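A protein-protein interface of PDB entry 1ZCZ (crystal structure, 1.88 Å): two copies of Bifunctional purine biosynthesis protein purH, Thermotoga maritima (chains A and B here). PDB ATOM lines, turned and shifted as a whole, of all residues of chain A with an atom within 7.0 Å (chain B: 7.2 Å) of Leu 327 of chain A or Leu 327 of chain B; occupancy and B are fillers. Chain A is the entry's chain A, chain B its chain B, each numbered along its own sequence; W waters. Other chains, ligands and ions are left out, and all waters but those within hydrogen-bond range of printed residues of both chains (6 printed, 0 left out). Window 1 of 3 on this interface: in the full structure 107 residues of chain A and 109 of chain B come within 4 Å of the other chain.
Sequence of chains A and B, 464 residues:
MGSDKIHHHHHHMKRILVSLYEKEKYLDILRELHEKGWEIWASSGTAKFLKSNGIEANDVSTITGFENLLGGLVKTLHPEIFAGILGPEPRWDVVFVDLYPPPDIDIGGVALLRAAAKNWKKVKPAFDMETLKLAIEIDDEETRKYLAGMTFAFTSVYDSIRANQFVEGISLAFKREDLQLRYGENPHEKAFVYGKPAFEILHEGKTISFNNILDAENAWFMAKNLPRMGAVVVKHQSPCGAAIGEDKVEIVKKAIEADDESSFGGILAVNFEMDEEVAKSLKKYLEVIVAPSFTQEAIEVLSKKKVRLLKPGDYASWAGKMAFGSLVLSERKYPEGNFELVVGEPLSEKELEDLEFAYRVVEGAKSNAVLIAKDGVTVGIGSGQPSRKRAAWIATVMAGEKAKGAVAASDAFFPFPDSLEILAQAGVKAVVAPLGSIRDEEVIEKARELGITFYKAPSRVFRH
Among the printed residues, merely in contact across the chains: Leu 172 of chain A with Leu 172 of chain B, Leu 172 of chain A with Tyr 194 of chain B, Phe 174 of chain A with Gly 325 of chain B, Phe 192 of chain A with Leu 327 of chain B, Phe 192 of chain A with Val 328 of chain B, Val 193 of chain A with Leu 327 of chain B, Tyr 194 of chain A with Leu 172 of chain B, Tyr 194 of chain A with Ser 326 of chain B, Phe 210 of chain A with Gly 320 of chain B, Phe 210 of chain A with Val 328 of chain B, Phe 210 of chain A with Leu 329 of chain B, Gly 320 of chain A with Phe 210 of chain B, Gly 320 of chain A with Lys 321 of chain B, Lys 321 of chain A with Gly 320 of chain B, Lys 321 of chain A with Lys 321 of chain B, Gly 325 of chain A with Phe 174 of chain B, Ser 326 of chain A with Tyr 194 of chain B, Ser 326 of chain A with Lys 196 of chain B, Leu 327 of chain A with Phe 192 of chain B, Leu 327 of chain A with Val 193 of chain B, Leu 327 of chain A with Leu 327 of chain B, Val 328 of chain A with Phe 192 of chain B, Val 328 of chain A with Phe 210 of chain B and Leu 329 of chain A with Phe 210 of chain B.
Of the 17 printed residues of chain A, 14 touch a printed residue of chain B. Among the printed residues, 32 pairs touch across the chains. Among the printed residues, no Asp or Glu carboxylate lies within 4 Å of a Lys or Arg side-chain nitrogen of the other chain.
The backbone carbonyl oxygen of Leu 172 of chain A sits at hydrogen-bond distance from the backbone NH of Phe 174 of chain B (2.8 Å). The backbone NH (N) of Phe 174 of chain A sits at hydrogen-bond distance from the backbone carbonyl oxygen (O) of Leu 172 of chain B, 2.9 Å away. N of Phe 192 of chain A lies within hydrogen-bond range of O of Leu 329 of chain B (2.8 Å). The backbone NH (N) of Leu 327 of chain B sits at hydrogen-bond distance from the backbone carbonyl oxygen (O) of Tyr 194 of chain A (2.9 Å). The backbone carbonyl oxygen (O) of Gly 195 of chain A sits at hydrogen-bond distance from the side-chain hydroxyl (OG) of Ser 326 of chain B. The side-chain hydroxyl (OG) of Ser 326 of chain A sits at hydrogen-bond distance from the backbone carbonyl oxygen (O) of Gly 195 of chain B (2.7 Å). The backbone carbonyl oxygen of Tyr 194 of chain B is in hydrogen-bond range of the backbone NH of Leu 327 of chain A (2.9 Å). The backbone carbonyl oxygen of Leu 329 of chain A lies within hydrogen-bond range of the backbone NH of Phe 192 of chain B, at 2.9 Å.
Water W1 lies within hydrogen-bond range of the backbone carbonyl oxygen of Gly 320 of chain A (2.7 Å) and the backbone NH of Met 322 of chain B (2.8 Å).
N of Val 328 of chain A sits at hydrogen-bond distance from O of Lys 321 of chain A (2.9 Å). The backbone NH (N) of Val 328 of chain B is in hydrogen-bond range of the backbone carbonyl oxygen (O) of Lys 321 of chain B (2.9 Å).
Phe 210 of chain A touches Val 328 of chain B, and with the chains exchanged Val 328 of chain A touches Phe 210 of chain B. Of the 32 pairs that touch across the chains among the printed residues, 31 have their exchanged pair printed and touching as well.
Of the printed residues of chain B, Gly 195 of chain A touches Ser 326 (2.8 Å). Phe 324 of chain A touches none of the printed residues of chain B. Of chain B, only Phe 192, Val 193, Tyr 194 and Leu 327 come within 4 Å of Leu 327 of chain A. Leu 327 of chain B touches just these residues of chain A: Phe 192 (3.7 Å), Val 193 (3.7 Å), Tyr 194 (2.9 Å) and Leu 327 (3.8 Å). The nearest residue of chain A that does not touch Leu 327 of chain B is Phe 174 of chain A (4.2 Å).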
ATOM      1  N   LEU A 172       6.482  27.954  -9.655  1.00  0.00           N
ATOM      2  CA  LEU A 172       6.444  26.726  -8.879  1.00  0.00           C
ATOM      3  C   LEU A 172       4.977  26.392  -8.599  1.00  0.00           C
ATOM      4  O   LEU A 172       4.218  27.248  -8.157  1.00  0.00           O
ATOM      5  CB  LEU A 172       7.246  26.873  -7.567  1.00  0.00           C
ATOM      6  CG  LEU A 172       7.385  25.636  -6.657  1.00  0.00           C
ATOM      7  CD1 LEU A 172       8.700  25.573  -5.942  1.00  0.00           C
ATOM      8  CD2 LEU A 172       6.249  25.599  -5.647  1.00  0.00           C
ATOM      9  N   PHE A 174       2.229  22.780  -7.567  1.00  0.00           N
ATOM     10  CA  PHE A 174       2.055  21.367  -7.254  1.00  0.00           C
ATOM     11  C   PHE A 174       0.583  21.109  -6.973  1.00  0.00           C
ATOM     12  O   PHE A 174      -0.129  21.998  -6.481  1.00  0.00           O
ATOM     13  CB  PHE A 174       2.795  21.011  -5.959  1.00  0.00           C
ATOM     14  CG  PHE A 174       4.277  20.902  -6.072  1.00  0.00           C
ATOM     15  CD1 PHE A 174       4.875  19.819  -6.690  1.00  0.00           C
ATOM     16  CD2 PHE A 174       5.083  21.844  -5.452  1.00  0.00           C
ATOM     17  CE1 PHE A 174       6.252  19.704  -6.711  1.00  0.00           C
ATOM     18  CE2 PHE A 174       6.453  21.733  -5.495  1.00  0.00           C
ATOM     19  CZ  PHE A 174       7.026  20.676  -6.114  1.00  0.00           C
ATOM     20  N   PHE A 192       0.610  18.583   4.941  1.00  0.00           N
ATOM     21  CA  PHE A 192       0.202  18.746   3.547  1.00  0.00           C
ATOM     22  C   PHE A 192       1.376  18.345   2.663  1.00  0.00           C
ATOM     23  O   PHE A 192       2.431  18.977   2.730  1.00  0.00           O
ATOM     24  CB  PHE A 192      -0.160  20.202   3.271  1.00  0.00           C
ATOM     25  CG  PHE A 192      -1.294  20.722   4.104  1.00  0.00           C
ATOM     26  CD1 PHE A 192      -1.059  21.286   5.358  1.00  0.00           C
ATOM     27  CD2 PHE A 192      -2.596  20.633   3.639  1.00  0.00           C
ATOM     28  CE1 PHE A 192      -2.129  21.759   6.139  1.00  0.00           C
ATOM     29  CE2 PHE A 192      -3.652  21.112   4.400  1.00  0.00           C
ATOM     30  CZ  PHE A 192      -3.418  21.672   5.652  1.00  0.00           C
ATOM     31  N   VAL A 193       1.172  17.355   1.793  1.00  0.00           N
ATOM     32  CA  VAL A 193       2.213  16.949   0.861  1.00  0.00           C
ATOM     33  C   VAL A 193       1.838  17.368  -0.552  1.00  0.00           C
ATOM     34  O   VAL A 193       0.734  17.077  -0.982  1.00  0.00           O
ATOM     35  CB  VAL A 193       2.450  15.436   0.912  1.00  0.00           C
ATOM     36  CG1 VAL A 193       3.505  15.010  -0.132  1.00  0.00           C
ATOM     37  CG2 VAL A 193       2.873  15.023   2.326  1.00  0.00           C
ATOM     38  N   TYR A 194       2.769  18.049  -1.232  1.00  0.00           N
ATOM     39  CA  TYR A 194       2.564  18.586  -2.578  1.00  0.00           C
ATOM     40  C   TYR A 194       3.509  17.971  -3.590  1.00  0.00           C
ATOM     41  O   TYR A 194       4.732  18.054  -3.457  1.00  0.00           O
ATOM     42  CB  TYR A 194       2.689  20.114  -2.566  1.00  0.00           C
ATOM     43  CG  TYR A 194       1.541  20.759  -1.837  1.00  0.00           C
ATOM     44  CD1 TYR A 194       0.299  20.890  -2.440  1.00  0.00           C
ATOM     45  CD2 TYR A 194       1.678  21.196  -0.514  1.00  0.00           C
ATOM     46  CE1 TYR A 194      -0.783  21.437  -1.765  1.00  0.00           C
ATOM     47  CE2 TYR A 194       0.590  21.730   0.177  1.00  0.00           C
ATOM     48  CZ  TYR A 194      -0.620  21.865  -0.443  1.00  0.00           C
ATOM     49  OH  TYR A 194      -1.717  22.371   0.183  1.00  0.00           O
ATOM     50  N   GLY A 195       2.913  17.364  -4.619  1.00  0.00           N
ATOM     51  CA  GLY A 195       3.620  16.623  -5.647  1.00  0.00           C
ATOM     52  C   GLY A 195       3.813  15.147  -5.307  1.00  0.00           C
ATOM     53  O   GLY A 195       3.935  14.787  -4.138  1.00  0.00           O
ATOM     54  N   PHE A 210       5.685  11.972   8.462  1.00  0.00           N
ATOM     55  CA  PHE A 210       6.282  13.235   8.056  1.00  0.00           C
ATOM     56  C   PHE A 210       7.766  13.294   8.433  1.00  0.00           C
ATOM     57  O   PHE A 210       8.610  13.606   7.587  1.00  0.00           O
ATOM     58  CB  PHE A 210       5.462  14.414   8.666  1.00  0.00           C
ATOM     59  CG  PHE A 210       6.031  15.770   8.408  1.00  0.00           C
ATOM     60  CD1 PHE A 210       6.953  16.313   9.284  1.00  0.00           C
ATOM     61  CD2 PHE A 210       5.622  16.542   7.326  1.00  0.00           C
ATOM     62  CE1 PHE A 210       7.505  17.535   9.056  1.00  0.00           C
ATOM     63  CE2 PHE A 210       6.201  17.797   7.104  1.00  0.00           C
ATOM     64  CZ  PHE A 210       7.111  18.284   7.984  1.00  0.00           C
ATOM     65  N   GLY A 320      16.178  24.627   2.155  1.00  0.00           N
ATOM     66  CA  GLY A 320      15.251  25.746   2.331  1.00  0.00           C
ATOM     67  C   GLY A 320      13.888  25.346   2.867  1.00  0.00           C
ATOM     68  O   GLY A 320      13.558  24.149   2.976  1.00  0.00           O
ATOM     69  N   LYS A 321      13.094  26.371   3.164  1.00  0.00           N
ATOM     70  CA  LYS A 321      11.836  26.219   3.884  1.00  0.00           C
ATOM     71  C   LYS A 321      10.898  27.375   3.579  1.00  0.00           C
ATOM     72  O   LYS A 321      11.319  28.370   2.984  1.00  0.00           O
ATOM     73  CB  LYS A 321      12.138  26.269   5.401  1.00  0.00           C
ATOM     74  CG  LYS A 321      12.827  25.082   5.976  1.00  0.00           C
ATOM     75  CD  LYS A 321      12.899  25.220   7.524  1.00  0.00           C
ATOM     76  CE  LYS A 321      13.462  23.992   8.219  1.00  0.00           C
ATOM     77  NZ  LYS A 321      13.577  24.290   9.679  1.00  0.00           N
ATOM     78  N   MET A 322       9.635  27.271   4.018  1.00  0.00           N
ATOM     79  CA  MET A 322       8.767  28.453   4.120  1.00  0.00           C
ATOM     80  C   MET A 322       9.318  29.417   5.164  1.00  0.00           C
ATOM     81  O   MET A 322       9.739  28.989   6.234  1.00  0.00           O
ATOM     82  CB  MET A 322       7.345  28.045   4.525  1.00  0.00           C
ATOM     83  CG  MET A 322       6.631  27.170   3.526  1.00  0.00           C
ATOM     84  SD  MET A 322       6.218  27.981   1.970  1.00  0.00           S
ATOM     85  CE  MET A 322       5.176  29.316   2.522  1.00  0.00           C
ATOM     86  N   ALA A 323       9.335  30.715   4.837  1.00  0.00           N
ATOM     87  CA  ALA A 323       9.733  31.758   5.751  1.00  0.00           C
ATOM     88  C   ALA A 323       8.982  32.995   5.353  1.00  0.00           C
ATOM     89  O   ALA A 323       8.982  33.352   4.172  1.00  0.00           O
ATOM     90  CB  ALA A 323      11.264  32.018   5.668  1.00  0.00           C
ATOM     91  N   PHE A 324       8.322  33.629   6.323  1.00  0.00           N
ATOM     92  CA  PHE A 324       7.527  34.842   6.098  1.00  0.00           C
ATOM     93  C   PHE A 324       6.522  34.689   4.944  1.00  0.00           C
ATOM     94  O   PHE A 324       6.228  35.660   4.240  1.00  0.00           O
ATOM     95  CB  PHE A 324       8.457  36.035   5.870  1.00  0.00           C
ATOM     96  CG  PHE A 324       9.421  36.254   7.000  1.00  0.00           C
ATOM     97  CD1 PHE A 324       9.051  36.985   8.104  1.00  0.00           C
ATOM     98  CD2 PHE A 324      10.689  35.669   6.965  1.00  0.00           C
ATOM     99  CE1 PHE A 324       9.960  37.165   9.171  1.00  0.00           C
ATOM    100  CE2 PHE A 324      11.591  35.862   8.007  1.00  0.00           C
ATOM    101  CZ  PHE A 324      11.233  36.597   9.081  1.00  0.00           C
ATOM    102  N   GLY A 325       6.011  33.468   4.788  1.00  0.00           N
ATOM    103  CA  GLY A 325       5.018  33.123   3.763  1.00  0.00           C
ATOM    104  C   GLY A 325       5.511  32.915   2.351  1.00  0.00           C
ATOM    105  O   GLY A 325       4.690  32.782   1.430  1.00  0.00           O
ATOM    106  N   SER A 326       6.837  32.926   2.176  1.00  0.00           N
ATOM    107  CA  SER A 326       7.516  32.667   0.904  1.00  0.00           C
ATOM    108  C   SER A 326       8.135  31.304   1.012  1.00  0.00           C
ATOM    109  O   SER A 326       8.528  30.889   2.103  1.00  0.00           O
ATOM    110  CB  SER A 326       8.627  33.717   0.603  1.00  0.00           C
ATOM    111  OG  SER A 326       8.096  35.012   0.452  1.00  0.00           O
ATOM    112  N   LEU A 327       8.236  30.577  -0.101  1.00  0.00           N
ATOM    113  CA  LEU A 327       9.078  29.371  -0.122  1.00  0.00           C
ATOM    114  C   LEU A 327      10.506  29.752  -0.548  1.00  0.00           C
ATOM    115  O   LEU A 327      10.733  30.177  -1.675  1.00  0.00           O
ATOM    116  CB  LEU A 327       8.484  28.332  -1.066  1.00  0.00           C
ATOM    117  CG  LEU A 327       9.208  27.006  -1.139  1.00  0.00           C
ATOM    118  CD1 LEU A 327       9.075  26.280   0.198  1.00  0.00           C
ATOM    119  CD2 LEU A 327       8.638  26.175  -2.257  1.00  0.00           C
ATOM    120  N   VAL A 328      11.470  29.602   0.368  1.00  0.00           N
ATOM    121  CA  VAL A 328      12.817  30.132   0.170  1.00  0.00           C
ATOM    122  C   VAL A 328      13.747  28.939  -0.026  1.00  0.00           C
ATOM    123  O   VAL A 328      14.097  28.280   0.939  1.00  0.00           O
ATOM    124  CB  VAL A 328      13.246  30.949   1.423  1.00  0.00           C
ATOM    125  CG1 VAL A 328      14.670  31.538   1.240  1.00  0.00           C
ATOM    126  CG2 VAL A 328      12.242  32.055   1.690  1.00  0.00           C
ATOM    127  N   LEU A 329      14.099  28.647  -1.268  1.00  0.00           N
ATOM    128  CA  LEU A 329      14.889  27.454  -1.630  1.00  0.00           C
ATOM    129  C   LEU A 329      16.300  27.779  -2.094  1.00  0.00           C
ATOM    130  O   LEU A 329      16.590  28.857  -2.583  1.00  0.00           O
ATOM    131  CB  LEU A 329      14.199  26.717  -2.765  1.00  0.00           C
ATOM    132  CG  LEU A 329      12.801  26.174  -2.458  1.00  0.00           C
ATOM    133  CD1 LEU A 329      12.304  25.498  -3.763  1.00  0.00           C
ATOM    134  CD2 LEU A 329      12.774  25.251  -1.259  1.00  0.00           C
ATOM    135  N   LEU B 172      -1.035  24.308  -4.740  1.00  0.00           N
ATOM    136  CA  LEU B 172      -0.055  25.233  -4.227  1.00  0.00           C
ATOM    137  C   LEU B 172       0.662  25.813  -5.432  1.00  0.00           C
ATOM    138  O   LEU B 172       1.071  25.081  -6.324  1.00  0.00           O
ATOM    139  CB  LEU B 172       0.915  24.529  -3.271  1.00  0.00           C
ATOM    140  CG  LEU B 172       2.021  25.357  -2.611  1.00  0.00           C
ATOM    141  CD1 LEU B 172       2.426  24.864  -1.244  1.00  0.00           C
ATOM    142  CD2 LEU B 172       3.233  25.385  -3.513  1.00  0.00           C
ATOM    143  N   PHE B 174       3.257  29.411  -6.746  1.00  0.00           N
ATOM    144  CA  PHE B 174       3.975  30.654  -6.432  1.00  0.00           C
ATOM    145  C   PHE B 174       4.598  31.195  -7.702  1.00  0.00           C
ATOM    146  O   PHE B 174       4.900  30.435  -8.623  1.00  0.00           O
ATOM    147  CB  PHE B 174       5.128  30.435  -5.451  1.00  0.00           C
ATOM    148  CG  PHE B 174       4.731  30.206  -4.019  1.00  0.00           C
ATOM    149  CD1 PHE B 174       4.392  31.263  -3.182  1.00  0.00           C
ATOM    150  CD2 PHE B 174       4.784  28.917  -3.473  1.00  0.00           C
ATOM    151  CE1 PHE B 174       4.075  31.040  -1.866  1.00  0.00           C
ATOM    152  CE2 PHE B 174       4.459  28.690  -2.155  1.00  0.00           C
ATOM    153  CZ  PHE B 174       4.109  29.760  -1.340  1.00  0.00           C
ATOM    154  N   PHE B 192      16.364  30.462  -4.990  1.00  0.00           N
ATOM    155  CA  PHE B 192      15.109  30.761  -5.641  1.00  0.00           C
ATOM    156  C   PHE B 192      14.101  31.083  -4.540  1.00  0.00           C
ATOM    157  O   PHE B 192      13.823  30.239  -3.685  1.00  0.00           O
ATOM    158  CB  PHE B 192      14.633  29.550  -6.439  1.00  0.00           C
ATOM    159  CG  PHE B 192      15.574  29.123  -7.519  1.00  0.00           C
ATOM    160  CD1 PHE B 192      16.641  28.272  -7.237  1.00  0.00           C
ATOM    161  CD2 PHE B 192      15.383  29.550  -8.825  1.00  0.00           C
ATOM    162  CE1 PHE B 192      17.523  27.888  -8.232  1.00  0.00           C
ATOM    163  CE2 PHE B 192      16.254  29.165  -9.830  1.00  0.00           C
ATOM    164  CZ  PHE B 192      17.329  28.333  -9.534  1.00  0.00           C
ATOM    165  N   VAL B 193      13.584  32.307  -4.546  1.00  0.00           N
ATOM    166  CA  VAL B 193      12.537  32.735  -3.626  1.00  0.00           C
ATOM    167  C   VAL B 193      11.184  32.822  -4.347  1.00  0.00           C
ATOM    168  O   VAL B 193      11.065  33.486  -5.376  1.00  0.00           O
ATOM    169  CB  VAL B 193      12.841  34.090  -3.046  1.00  0.00           C
ATOM    170  CG1 VAL B 193      11.748  34.498  -2.083  1.00  0.00           C
ATOM    171  CG2 VAL B 193      14.221  34.069  -2.350  1.00  0.00           C
ATOM    172  N   TYR B 194      10.171  32.178  -3.769  1.00  0.00           N
ATOM    173  CA  TYR B 194       8.866  32.055  -4.371  1.00  0.00           C
ATOM    174  C   TYR B 194       7.847  32.733  -3.492  1.00  0.00           C
ATOM    175  O   TYR B 194       7.747  32.421  -2.296  1.00  0.00           O
ATOM    176  CB  TYR B 194       8.521  30.574  -4.576  1.00  0.00           C
ATOM    177  CG  TYR B 194       9.326  30.001  -5.715  1.00  0.00           C
ATOM    178  CD1 TYR B 194       8.987  30.282  -7.037  1.00  0.00           C
ATOM    179  CD2 TYR B 194      10.458  29.235  -5.481  1.00  0.00           C
ATOM    180  CE1 TYR B 194       9.762  29.766  -8.095  1.00  0.00           C
ATOM    181  CE2 TYR B 194      11.209  28.715  -6.513  1.00  0.00           C
ATOM    182  CZ  TYR B 194      10.864  28.992  -7.822  1.00  0.00           C
ATOM    183  OH  TYR B 194      11.641  28.520  -8.836  1.00  0.00           O
ATOM    184  N   GLY B 195       7.098  33.668  -4.091  1.00  0.00           N
ATOM    185  CA  GLY B 195       6.117  34.456  -3.362  1.00  0.00           C
ATOM    186  C   GLY B 195       6.713  35.649  -2.632  1.00  0.00           C
ATOM    187  O   GLY B 195       7.857  35.610  -2.172  1.00  0.00           O
ATOM    188  N   LYS B 196       5.938  36.715  -2.504  1.00  0.00           N
ATOM    189  CA  LYS B 196       6.426  37.894  -1.822  1.00  0.00           C
ATOM    190  C   LYS B 196       6.445  37.662  -0.325  1.00  0.00           C
ATOM    191  O   LYS B 196       5.408  37.351   0.254  1.00  0.00           O
ATOM    192  CB  LYS B 196       5.571  39.135  -2.126  1.00  0.00           C
ATOM    193  CG  LYS B 196       6.195  40.455  -1.618  1.00  0.00           C
ATOM    194  CD  LYS B 196       5.641  41.716  -2.312  1.00  0.00           C
ATOM    195  CE  LYS B 196       6.518  42.957  -2.018  1.00  0.00           C
ATOM    196  NZ  LYS B 196       6.068  44.212  -2.739  1.00  0.00           N
ATOM    197  N   PHE B 210      20.134  34.484   2.156  1.00  0.00           N
ATOM    198  CA  PHE B 210      19.305  33.283   2.318  1.00  0.00           C
ATOM    199  C   PHE B 210      19.299  32.822   3.781  1.00  0.00           C
ATOM    200  O   PHE B 210      18.237  32.625   4.376  1.00  0.00           O
ATOM    201  CB  PHE B 210      19.851  32.202   1.364  1.00  0.00           C
ATOM    202  CG  PHE B 210      19.175  30.886   1.483  1.00  0.00           C
ATOM    203  CD1 PHE B 210      19.584  29.967   2.446  1.00  0.00           C
ATOM    204  CD2 PHE B 210      18.166  30.541   0.617  1.00  0.00           C
ATOM    205  CE1 PHE B 210      18.949  28.723   2.589  1.00  0.00           C
ATOM    206  CE2 PHE B 210      17.526  29.312   0.748  1.00  0.00           C
ATOM    207  CZ  PHE B 210      17.923  28.405   1.754  1.00  0.00           C
ATOM    208  N   ALA B 319       6.476  24.279   9.071  1.00  0.00           N
ATOM    209  CA  ALA B 319       7.601  23.388   9.083  1.00  0.00           C
ATOM    210  C   ALA B 319       7.606  22.571   7.756  1.00  0.00           C
ATOM    211  O   ALA B 319       6.611  22.481   7.055  1.00  0.00           O
ATOM    212  CB  ALA B 319       7.539  22.454  10.276  1.00  0.00           C
ATOM    213  N   GLY B 320       8.742  21.953   7.485  1.00  0.00           N
ATOM    214  CA  GLY B 320       8.909  21.108   6.321  1.00  0.00           C
ATOM    215  C   GLY B 320       9.838  21.645   5.257  1.00  0.00           C
ATOM    216  O   GLY B 320      10.371  22.758   5.356  1.00  0.00           O
ATOM    217  N   LYS B 321      10.062  20.814   4.233  1.00  0.00           N
ATOM    218  CA  LYS B 321      11.076  21.059   3.205  1.00  0.00           C
ATOM    219  C   LYS B 321      10.697  20.275   1.955  1.00  0.00           C
ATOM    220  O   LYS B 321       9.783  19.434   1.986  1.00  0.00           O
ATOM    221  CB  LYS B 321      12.448  20.553   3.661  1.00  0.00           C
ATOM    222  CG  LYS B 321      13.091  21.283   4.822  1.00  0.00           C
ATOM    223  CD  LYS B 321      14.563  20.805   4.991  1.00  0.00           C
ATOM    224  CE  LYS B 321      15.300  21.591   6.087  1.00  0.00           C
ATOM    225  NZ  LYS B 321      16.578  20.902   6.414  1.00  0.00           N
ATOM    226  N   MET B 322      11.438  20.506   0.886  1.00  0.00           N
ATOM    227  CA  MET B 322      11.433  19.599  -0.268  1.00  0.00           C
ATOM    228  C   MET B 322      12.094  18.287   0.143  1.00  0.00           C
ATOM    229  O   MET B 322      13.101  18.299   0.829  1.00  0.00           O
ATOM    230  CB  MET B 322      12.241  20.208  -1.428  1.00  0.00           C
ATOM    231  CG  MET B 322      11.604  21.490  -2.040  1.00  0.00           C
ATOM    232  SD  MET B 322      10.037  21.181  -2.889  1.00  0.00           S
ATOM    233  CE  MET B 322      10.550  20.053  -4.139  1.00  0.00           C
ATOM    234  N   ALA B 323      11.518  17.180  -0.272  1.00  0.00           N
ATOM    235  CA  ALA B 323      12.076  15.845  -0.044  1.00  0.00           C
ATOM    236  C   ALA B 323      11.582  14.945  -1.143  1.00  0.00           C
ATOM    237  O   ALA B 323      10.378  14.873  -1.374  1.00  0.00           O
ATOM    238  CB  ALA B 323      11.612  15.293   1.302  1.00  0.00           C
ATOM    239  N   PHE B 324      12.496  14.220  -1.792  1.00  0.00           N
ATOM    240  CA  PHE B 324      12.129  13.324  -2.885  1.00  0.00           C
ATOM    241  C   PHE B 324      11.308  14.035  -3.983  1.00  0.00           C
ATOM    242  O   PHE B 324      10.477  13.407  -4.667  1.00  0.00           O
ATOM    243  CB  PHE B 324      11.423  12.088  -2.329  1.00  0.00           C
ATOM    244  CG  PHE B 324      12.245  11.331  -1.306  1.00  0.00           C
ATOM    245  CD1 PHE B 324      13.193  10.402  -1.722  1.00  0.00           C
ATOM    246  CD2 PHE B 324      12.075  11.565   0.058  1.00  0.00           C
ATOM    247  CE1 PHE B 324      13.970   9.707  -0.797  1.00  0.00           C
ATOM    248  CE2 PHE B 324      12.862  10.865   1.014  1.00  0.00           C
ATOM    249  CZ  PHE B 324      13.814   9.945   0.564  1.00  0.00           C
ATOM    250  N   GLY B 325      11.598  15.324  -4.189  1.00  0.00           N
ATOM    251  CA  GLY B 325      10.907  16.129  -5.205  1.00  0.00           C
ATOM    252  C   GLY B 325       9.471  16.560  -4.880  1.00  0.00           C
ATOM    253  O   GLY B 325       8.782  17.074  -5.763  1.00  0.00           O
ATOM    254  N   SER B 326       9.045  16.373  -3.626  1.00  0.00           N
ATOM    255  CA  SER B 326       7.752  16.828  -3.128  1.00  0.00           C
ATOM    256  C   SER B 326       8.021  17.890  -2.123  1.00  0.00           C
ATOM    257  O   SER B 326       9.053  17.831  -1.487  1.00  0.00           O
ATOM    258  CB  SER B 326       6.989  15.700  -2.415  1.00  0.00           C
ATOM    259  OG  SER B 326       6.607  14.700  -3.320  1.00  0.00           O
ATOM    260  N   LEU B 327       7.104  18.850  -1.973  1.00  0.00           N
ATOM    261  CA  LEU B 327       7.161  19.805  -0.865  1.00  0.00           C
ATOM    262  C   LEU B 327       6.343  19.257   0.289  1.00  0.00           C
ATOM    263  O   LEU B 327       5.129  19.117   0.186  1.00  0.00           O
ATOM    264  CB  LEU B 327       6.598  21.159  -1.288  1.00  0.00           C
ATOM    265  CG  LEU B 327       6.656  22.301  -0.268  1.00  0.00           C
ATOM    266  CD1 LEU B 327       8.098  22.574   0.086  1.00  0.00           C
ATOM    267  CD2 LEU B 327       6.022  23.587  -0.833  1.00  0.00           C
ATOM    268  N   VAL B 328       7.004  18.961   1.398  1.00  0.00           N
ATOM    269  CA  VAL B 328       6.384  18.230   2.485  1.00  0.00           C
ATOM    270  C   VAL B 328       6.261  19.167   3.649  1.00  0.00           C
ATOM    271  O   VAL B 328       7.282  19.532   4.231  1.00  0.00           O
ATOM    272  CB  VAL B 328       7.252  16.992   2.827  1.00  0.00           C
ATOM    273  CG1 VAL B 328       6.683  16.232   3.988  1.00  0.00           C
ATOM    274  CG2 VAL B 328       7.370  16.106   1.609  1.00  0.00           C
ATOM    275  N   LEU B 329       5.037  19.616   3.926  1.00  0.00           N
ATOM    276  CA  LEU B 329       4.791  20.716   4.883  1.00  0.00           C
ATOM    277  C   LEU B 329       3.937  20.319   6.068  1.00  0.00           C
ATOM    278  O   LEU B 329       3.095  19.425   5.982  1.00  0.00           O
ATOM    279  CB  LEU B 329       4.033  21.851   4.191  1.00  0.00           C
ATOM    280  CG  LEU B 329       4.728  22.606   3.059  1.00  0.00           C
ATOM    281  CD1 LEU B 329       3.801  23.750   2.615  1.00  0.00           C
ATOM    282  CD2 LEU B 329       6.107  23.098   3.483  1.00  0.00           C
HETATM  283  O   HOH W   1      13.549  22.363   0.924  1.00  0.00           O
HETATM  284  O   HOH W   2      -0.988  24.296  -8.593  1.00  0.00           O
HETATM  285  O   HOH W   3       8.772  25.044   5.670  1.00  0.00           O
HETATM  286  O   HOH W   4       4.162  34.539  -0.444  1.00  0.00           O
HETATM  287  O   HOH W   5      16.093  22.213   9.217  1.00  0.00           O
HETATM  288  O   HOH W   6       4.111  36.098   2.483  1.00  0.00           O
